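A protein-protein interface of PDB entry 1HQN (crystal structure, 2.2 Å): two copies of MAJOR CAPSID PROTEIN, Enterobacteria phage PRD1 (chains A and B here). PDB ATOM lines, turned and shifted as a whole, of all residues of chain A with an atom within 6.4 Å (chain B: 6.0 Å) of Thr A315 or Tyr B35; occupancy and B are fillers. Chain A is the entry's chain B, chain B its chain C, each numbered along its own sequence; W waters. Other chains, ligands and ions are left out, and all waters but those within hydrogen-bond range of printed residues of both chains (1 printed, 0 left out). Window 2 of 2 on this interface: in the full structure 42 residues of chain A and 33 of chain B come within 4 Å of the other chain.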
ATOM      1  N   SER A 306     -33.029  23.600  25.221  1.00  0.00           N
ATOM      2  CA  SER A 306     -31.616  23.898  25.291  1.00  0.00           C
ATOM      3  C   SER A 306     -31.348  25.331  25.699  1.00  0.00           C
ATOM      4  O   SER A 306     -32.264  26.137  25.843  1.00  0.00           O
ATOM      5  CB  SER A 306     -30.974  23.633  23.920  1.00  0.00           C
ATOM      6  OG  SER A 306     -29.575  23.853  23.938  1.00  0.00           O
ATOM      7  N   GLN A 307     -30.069  25.615  25.903  1.00  0.00           N
ATOM      8  CA  GLN A 307     -29.560  26.940  26.229  1.00  0.00           C
ATOM      9  C   GLN A 307     -28.371  27.047  25.285  1.00  0.00           C
ATOM     10  O   GLN A 307     -27.430  26.260  25.388  1.00  0.00           O
ATOM     11  CB  GLN A 307     -29.058  27.023  27.672  1.00  0.00           C
ATOM     12  CG  GLN A 307     -30.129  27.053  28.738  1.00  0.00           C
ATOM     13  CD  GLN A 307     -29.586  27.543  30.071  1.00  0.00           C
ATOM     14  OE1 GLN A 307     -28.582  27.033  30.569  1.00  0.00           O
ATOM     15  NE2 GLN A 307     -30.248  28.537  30.652  1.00  0.00           N
ATOM     16  N   ARG A 308     -28.412  27.992  24.354  1.00  0.00           N
ATOM     17  CA  ARG A 308     -27.311  28.131  23.408  1.00  0.00           C
ATOM     18  C   ARG A 308     -26.787  29.553  23.300  1.00  0.00           C
ATOM     19  O   ARG A 308     -27.454  30.508  23.688  1.00  0.00           O
ATOM     20  CB  ARG A 308     -27.742  27.650  22.019  1.00  0.00           C
ATOM     21  CG  ARG A 308     -28.820  28.504  21.377  1.00  0.00           C
ATOM     22  CD  ARG A 308     -29.128  28.044  19.958  1.00  0.00           C
ATOM     23  NE  ARG A 308     -29.477  26.626  19.901  1.00  0.00           N
ATOM     24  CZ  ARG A 308     -30.339  26.109  19.031  1.00  0.00           C
ATOM     25  NH1 ARG A 308     -30.943  26.895  18.147  1.00  0.00           N
ATOM     26  NH2 ARG A 308     -30.603  24.809  19.044  1.00  0.00           N
ATOM     27  N   THR A 309     -25.580  29.677  22.762  1.00  0.00           N
ATOM     28  CA  THR A 309     -24.948  30.975  22.577  1.00  0.00           C
ATOM     29  C   THR A 309     -24.930  31.334  21.095  1.00  0.00           C
ATOM     30  O   THR A 309     -25.133  30.473  20.240  1.00  0.00           O
ATOM     31  CB  THR A 309     -23.506  30.962  23.106  1.00  0.00           C
ATOM     32  OG1 THR A 309     -23.525  30.688  24.512  1.00  0.00           O
ATOM     33  CG2 THR A 309     -22.829  32.307  22.867  1.00  0.00           C
ATOM     34  N   SER A 313     -23.682  27.189  19.828  1.00  0.00           N
ATOM     35  CA  SER A 313     -23.086  26.116  20.615  1.00  0.00           C
ATOM     36  C   SER A 313     -24.054  25.020  21.073  1.00  0.00           C
ATOM     37  O   SER A 313     -24.082  23.928  20.495  1.00  0.00           O
ATOM     38  CB  SER A 313     -22.375  26.709  21.839  1.00  0.00           C
ATOM     39  OG  SER A 313     -21.375  27.641  21.457  1.00  0.00           O
ATOM     40  N   ASP A 314     -24.837  25.329  22.107  1.00  0.00           N
ATOM     41  CA  ASP A 314     -25.794  24.401  22.725  1.00  0.00           C
ATOM     42  C   ASP A 314     -25.082  23.659  23.856  1.00  0.00           C
ATOM     43  O   ASP A 314     -24.566  22.555  23.665  1.00  0.00           O
ATOM     44  CB  ASP A 314     -26.360  23.380  21.725  1.00  0.00           C
ATOM     45  CG  ASP A 314     -27.515  23.934  20.903  1.00  0.00           C
ATOM     46  OD1 ASP A 314     -28.469  24.478  21.496  1.00  0.00           O
ATOM     47  OD2 ASP A 314     -27.473  23.810  19.659  1.00  0.00           O
ATOM     48  N   THR A 315     -25.052  24.283  25.029  1.00  0.00           N
ATOM     49  CA  THR A 315     -24.407  23.703  26.200  1.00  0.00           C
ATOM     50  C   THR A 315     -25.305  22.678  26.891  1.00  0.00           C
ATOM     51  O   THR A 315     -24.840  21.907  27.733  1.00  0.00           O
ATOM     52  CB  THR A 315     -24.043  24.794  27.233  1.00  0.00           C
ATOM     53  OG1 THR A 315     -25.234  25.464  27.662  1.00  0.00           O
ATOM     54  CG2 THR A 315     -23.098  25.814  26.625  1.00  0.00           C
ATOM     55  N   ARG A 316     -26.586  22.672  26.524  1.00  0.00           N
ATOM     56  CA  ARG A 316     -27.559  21.760  27.120  1.00  0.00           C
ATOM     57  C   ARG A 316     -28.683  21.343  26.171  1.00  0.00           C
ATOM     58  O   ARG A 316     -29.854  21.466  26.526  1.00  0.00           O
ATOM     59  CB  ARG A 316     -28.215  22.407  28.348  1.00  0.00           C
ATOM     60  CG  ARG A 316     -27.358  22.512  29.586  1.00  0.00           C
ATOM     61  CD  ARG A 316     -28.198  22.973  30.787  1.00  0.00           C
ATOM     62  NE  ARG A 316     -29.398  22.153  30.957  1.00  0.00           N
ATOM     63  CZ  ARG A 316     -30.045  21.980  32.108  1.00  0.00           C
ATOM     64  NH1 ARG A 316     -29.614  22.567  33.218  1.00  0.00           N
ATOM     65  NH2 ARG A 316     -31.133  21.217  32.145  1.00  0.00           N
ATOM     66  N   LYS A 317     -28.365  20.865  24.975  1.00  0.00           N
ATOM     67  CA  LYS A 317     -29.439  20.444  24.076  1.00  0.00           C
ATOM     68  C   LYS A 317     -29.894  19.064  24.563  1.00  0.00           C
ATOM     69  O   LYS A 317     -29.175  18.078  24.407  1.00  0.00           O
ATOM     70  CB  LYS A 317     -28.936  20.376  22.637  1.00  0.00           C
ATOM     71  CG  LYS A 317     -30.026  20.092  21.625  1.00  0.00           C
ATOM     72  CD  LYS A 317     -29.451  20.029  20.217  1.00  0.00           C
ATOM     73  CE  LYS A 317     -30.526  19.698  19.194  1.00  0.00           C
ATOM     74  NZ  LYS A 317     -29.945  19.470  17.836  1.00  0.00           N
ATOM     75  N   ASN A 344     -29.021  27.700  36.833  1.00  0.00           N
ATOM     76  CA  ASN A 344     -27.772  28.346  36.406  1.00  0.00           C
ATOM     77  C   ASN A 344     -27.212  29.129  37.595  1.00  0.00           C
ATOM     78  O   ASN A 344     -26.619  30.198  37.425  1.00  0.00           O
ATOM     79  CB  ASN A 344     -28.022  29.316  35.244  1.00  0.00           C
ATOM     80  CG  ASN A 344     -28.378  28.610  33.956  1.00  0.00           C
ATOM     81  OD1 ASN A 344     -27.541  27.942  33.349  1.00  0.00           O
ATOM     82  ND2 ASN A 344     -29.624  28.750  33.529  1.00  0.00           N
ATOM     83  N   LYS A 347     -23.098  29.359  37.719  1.00  0.00           N
ATOM     84  CA  LYS A 347     -22.584  30.184  36.627  1.00  0.00           C
ATOM     85  C   LYS A 347     -23.763  30.877  35.954  1.00  0.00           C
ATOM     86  O   LYS A 347     -24.228  30.449  34.902  1.00  0.00           O
ATOM     87  CB  LYS A 347     -21.842  29.316  35.604  1.00  0.00           C
ATOM     88  CG  LYS A 347     -20.633  28.583  36.178  1.00  0.00           C
ATOM     89  CD  LYS A 347     -19.964  27.704  35.130  1.00  0.00           C
ATOM     90  CE  LYS A 347     -18.796  26.926  35.721  1.00  0.00           C
ATOM     91  NZ  LYS A 347     -17.720  27.821  36.231  1.00  0.00           N
ATOM     92  N   ILE A 349     -26.310  33.036  33.815  1.00  0.00           N
ATOM     93  CA  ILE A 349     -26.294  33.459  32.419  1.00  0.00           C
ATOM     94  C   ILE A 349     -26.088  34.968  32.459  1.00  0.00           C
ATOM     95  O   ILE A 349     -26.862  35.694  33.086  1.00  0.00           O
ATOM     96  CB  ILE A 349     -27.629  33.157  31.713  1.00  0.00           C
ATOM     97  CG1 ILE A 349     -27.946  31.661  31.799  1.00  0.00           C
ATOM     98  CG2 ILE A 349     -27.563  33.621  30.262  1.00  0.00           C
ATOM     99  CD1 ILE A 349     -26.918  30.775  31.143  1.00  0.00           C
ATOM    100  N   VAL B  30      -9.665  25.452  36.825  1.00  0.00           N
ATOM    101  CA  VAL B  30     -10.380  24.828  35.713  1.00  0.00           C
ATOM    102  C   VAL B  30     -11.897  24.892  35.920  1.00  0.00           C
ATOM    103  O   VAL B  30     -12.638  25.240  35.003  1.00  0.00           O
ATOM    104  CB  VAL B  30      -9.961  23.352  35.532  1.00  0.00           C
ATOM    105  CG1 VAL B  30     -10.908  22.653  34.565  1.00  0.00           C
ATOM    106  CG2 VAL B  30      -8.543  23.284  35.000  1.00  0.00           C
ATOM    107  N   GLN B  33     -12.877  28.702  35.389  1.00  0.00           N
ATOM    108  CA  GLN B  33     -12.698  29.295  34.061  1.00  0.00           C
ATOM    109  C   GLN B  33     -13.394  28.604  32.887  1.00  0.00           C
ATOM    110  O   GLN B  33     -13.878  29.272  31.970  1.00  0.00           O
ATOM    111  CB  GLN B  33     -11.202  29.412  33.739  1.00  0.00           C
ATOM    112  CG  GLN B  33     -10.382  30.150  34.793  1.00  0.00           C
ATOM    113  CD  GLN B  33     -11.029  31.449  35.236  1.00  0.00           C
ATOM    114  OE1 GLN B  33     -11.541  32.210  34.414  1.00  0.00           O
ATOM    115  NE2 GLN B  33     -11.000  31.714  36.541  1.00  0.00           N
ATOM    116  N   SER B  34     -13.430  27.275  32.898  1.00  0.00           N
ATOM    117  CA  SER B  34     -14.064  26.526  31.815  1.00  0.00           C
ATOM    118  C   SER B  34     -15.579  26.496  31.988  1.00  0.00           C
ATOM    119  O   SER B  34     -16.096  26.854  33.047  1.00  0.00           O
ATOM    120  CB  SER B  34     -13.530  25.093  31.785  1.00  0.00           C
ATOM    121  OG  SER B  34     -13.860  24.402  32.978  1.00  0.00           O
ATOM    122  N   TYR B  35     -16.296  26.081  30.950  1.00  0.00           N
ATOM    123  CA  TYR B  35     -17.749  26.001  31.058  1.00  0.00           C
ATOM    124  C   TYR B  35     -18.196  24.567  30.835  1.00  0.00           C
ATOM    125  O   TYR B  35     -17.788  23.922  29.867  1.00  0.00           O
ATOM    126  CB  TYR B  35     -18.445  26.908  30.035  1.00  0.00           C
ATOM    127  CG  TYR B  35     -19.919  27.128  30.345  1.00  0.00           C
ATOM    128  CD1 TYR B  35     -20.316  27.925  31.427  1.00  0.00           C
ATOM    129  CD2 TYR B  35     -20.915  26.515  29.577  1.00  0.00           C
ATOM    130  CE1 TYR B  35     -21.672  28.104  31.740  1.00  0.00           C
ATOM    131  CE2 TYR B  35     -22.278  26.688  29.882  1.00  0.00           C
ATOM    132  CZ  TYR B  35     -22.646  27.484  30.964  1.00  0.00           C
ATOM    133  OH  TYR B  35     -23.983  27.663  31.260  1.00  0.00           O
ATOM    134  N   PRO B  36     -19.048  24.047  31.732  1.00  0.00           N
ATOM    135  CA  PRO B  36     -19.546  22.675  31.616  1.00  0.00           C
ATOM    136  C   PRO B  36     -20.474  22.513  30.420  1.00  0.00           C
ATOM    137  O   PRO B  36     -21.278  23.396  30.118  1.00  0.00           O
ATOM    138  CB  PRO B  36     -20.268  22.460  32.944  1.00  0.00           C
ATOM    139  CG  PRO B  36     -20.823  23.829  33.233  1.00  0.00           C
ATOM    140  CD  PRO B  36     -19.642  24.726  32.898  1.00  0.00           C
ATOM    141  N   VAL B  37     -20.359  21.380  29.740  1.00  0.00           N
ATOM    142  CA  VAL B  37     -21.190  21.106  28.583  1.00  0.00           C
ATOM    143  C   VAL B  37     -21.634  19.653  28.557  1.00  0.00           C
ATOM    144  O   VAL B  37     -20.891  18.763  28.950  1.00  0.00           O
ATOM    145  CB  VAL B  37     -20.429  21.394  27.271  1.00  0.00           C
ATOM    146  CG1 VAL B  37     -21.278  20.999  26.070  1.00  0.00           C
ATOM    147  CG2 VAL B  37     -20.057  22.863  27.199  1.00  0.00           C
ATOM    148  N   ILE B  38     -22.868  19.429  28.124  1.00  0.00           N
ATOM    149  CA  ILE B  38     -23.396  18.084  27.969  1.00  0.00           C
ATOM    150  C   ILE B  38     -24.059  18.092  26.599  1.00  0.00           C
ATOM    151  O   ILE B  38     -24.936  18.917  26.332  1.00  0.00           O
ATOM    152  CB  ILE B  38     -24.427  17.691  29.070  1.00  0.00           C
ATOM    153  CG1 ILE B  38     -24.881  16.249  28.836  1.00  0.00           C
ATOM    154  CG2 ILE B  38     -25.635  18.605  29.046  1.00  0.00           C
ATOM    155  CD1 ILE B  38     -25.691  15.659  29.962  1.00  0.00           C
ATOM    156  N   GLN B  39     -23.606  17.201  25.721  1.00  0.00           N
ATOM    157  CA  GLN B  39     -24.146  17.116  24.369  1.00  0.00           C
ATOM    158  C   GLN B  39     -24.289  15.672  23.911  1.00  0.00           C
ATOM    159  O   GLN B  39     -23.497  14.812  24.296  1.00  0.00           O
ATOM    160  CB  GLN B  39     -23.238  17.865  23.393  1.00  0.00           C
ATOM    161  CG  GLN B  39     -21.811  17.349  23.354  1.00  0.00           C
ATOM    162  CD  GLN B  39     -20.941  18.095  22.348  1.00  0.00           C
ATOM    163  OE1 GLN B  39     -20.858  19.324  22.368  1.00  0.00           O
ATOM    164  NE2 GLN B  39     -20.276  17.349  21.472  1.00  0.00           N
ATOM    165  N   TYR B 235     -18.649  17.228  29.642  1.00  0.00           N
ATOM    166  CA  TYR B 235     -17.259  17.670  29.660  1.00  0.00           C
ATOM    167  C   TYR B 235     -17.091  19.157  29.950  1.00  0.00           C
ATOM    168  O   TYR B 235     -18.066  19.910  30.016  1.00  0.00           O
ATOM    169  CB  TYR B 235     -16.592  17.333  28.321  1.00  0.00           C
ATOM    170  CG  TYR B 235     -17.161  18.073  27.130  1.00  0.00           C
ATOM    171  CD1 TYR B 235     -18.229  17.542  26.405  1.00  0.00           C
ATOM    172  CD2 TYR B 235     -16.617  19.291  26.710  1.00  0.00           C
ATOM    173  CE1 TYR B 235     -18.744  18.202  25.286  1.00  0.00           C
ATOM    174  CE2 TYR B 235     -17.123  19.962  25.587  1.00  0.00           C
ATOM    175  CZ  TYR B 235     -18.186  19.408  24.881  1.00  0.00           C
ATOM    176  OH  TYR B 235     -18.684  20.039  23.765  1.00  0.00           O
ATOM    177  N   LEU B 236     -15.840  19.566  30.131  1.00  0.00           N
ATOM    178  CA  LEU B 236     -15.514  20.959  30.404  1.00  0.00           C
ATOM    179  C   LEU B 236     -14.885  21.559  29.154  1.00  0.00           C
ATOM    180  O   LEU B 236     -13.910  21.032  28.614  1.00  0.00           O
ATOM    181  CB  LEU B 236     -14.559  21.066  31.596  1.00  0.00           C
ATOM    182  CG  LEU B 236     -15.123  20.593  32.942  1.00  0.00           C
ATOM    183  CD1 LEU B 236     -14.076  20.784  34.026  1.00  0.00           C
ATOM    184  CD2 LEU B 236     -16.386  21.375  33.289  1.00  0.00           C
ATOM    185  N   ASP B 237     -15.455  22.663  28.690  1.00  0.00           N
ATOM    186  CA  ASP B 237     -14.970  23.316  27.484  1.00  0.00           C
ATOM    187  C   ASP B 237     -14.249  24.635  27.779  1.00  0.00           C
ATOM    188  O   ASP B 237     -14.400  25.214  28.862  1.00  0.00           O
ATOM    189  CB  ASP B 237     -16.151  23.542  26.537  1.00  0.00           C
ATOM    190  CG  ASP B 237     -15.752  23.465  25.082  1.00  0.00           C
ATOM    191  OD1 ASP B 237     -14.762  22.769  24.773  1.00  0.00           O
ATOM    192  OD2 ASP B 237     -16.437  24.087  24.244  1.00  0.00           O
ATOM    193  N   GLN B 238     -13.465  25.096  26.805  1.00  0.00           N
ATOM    194  CA  GLN B 238     -12.695  26.337  26.927  1.00  0.00           C
ATOM    195  C   GLN B 238     -11.789  26.270  28.144  1.00  0.00           C
ATOM    196  O   GLN B 238     -11.935  27.049  29.088  1.00  0.00           O
ATOM    197  CB  GLN B 238     -13.624  27.543  27.048  1.00  0.00           C
ATOM    198  CG  GLN B 238     -14.486  27.778  25.827  1.00  0.00           C
ATOM    199  CD  GLN B 238     -15.248  29.086  25.907  1.00  0.00           C
ATOM    200  OE1 GLN B 238     -15.969  29.342  26.879  1.00  0.00           O
ATOM    201  NE2 GLN B 238     -15.094  29.924  24.886  1.00  0.00           N
HETATM  202  O   HOH W   1     -24.186  22.610  30.603  1.00  0.00           O
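O of Thr A315 is in hydrogen-bond range of N of Ile B38 (3.2 Å).
The backbone carbonyl oxygen (O) of Tyr B35 sits at hydrogen-bond distance from the backbone NH (N) of Asp B237.
The backbone carbonyl oxygen (O) of Tyr B235 sits at hydrogen-bond distance from the backbone NH (N) of Val B37.
O of Gln A307 sits at hydrogen-bond distance from N of Thr A315, at 3.1 Å.
The side-chain hydroxyl (OG) of Ser B34 is in hydrogen-bond range of the backbone carbonyl oxygen (O) of Val B30 (2.5 Å).
Among the printed residues, merely in contact across the chains: Thr A315 with Tyr B35 (3.5 Å), Thr A315 with Val B37 (3.8 Å), Arg A316 with Ile B38 (3.9 Å), Lys A347 with Ser B34 (3.7 Å), Lys A347 with Tyr B35 (3.7 Å) and Lys A347 with Pro B36 (3.7 Å).
Thr A315 touches three residues of chain B.
Printed residues of chain B within 4 Å of Arg A316: Ile B38.
Of the printed residues of chain B, Lys A347 touches Ser B34 (3.7 Å), Tyr B35 (3.7 Å) and Pro B36 (3.7 Å).
Of the printed residues of chain A, Ser B34 touches Lys A347.
Of chain A, only Thr A315 and Lys A347 come within 4 Å of Tyr B35.
Of the printed residues of chain A, Pro B36 touches Lys A347.
Printed residues of chain A within 4 Å of Val B37: Thr A315.
The nearest residue of chain B that does not touch Thr A315 is Pro B36 (4.2 Å).
The nearest printed residue of chain A that does not touch Ile B38 is Lys A317 (4.2 Å).
Printed residues of chain A that touch a printed residue of chain B: Thr A315, Arg A316 and Lys A347.
Printed residues of chain B that touch a printed residue of chain A: Ser B34, Tyr B35, Pro B36, Val B37 and Ile B38.
Hydrophobic or aromatic side chains of chain B within 4 Å of the printed part of chain A: Tyr B35, Pro B36 and Ile B38.
Among the printed residues, 7 pairs touch across the chains.
Among the printed residues, no Asp or Glu carboxylate lies within 4 Å of a Lys or Arg side-chain nitrogen of the other chain.
No position is printed for both chains.
Water W1 bridges the backbone carbonyl oxygen (O) of Thr A315 and the backbone carbonyl oxygen (O) of Pro B36.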
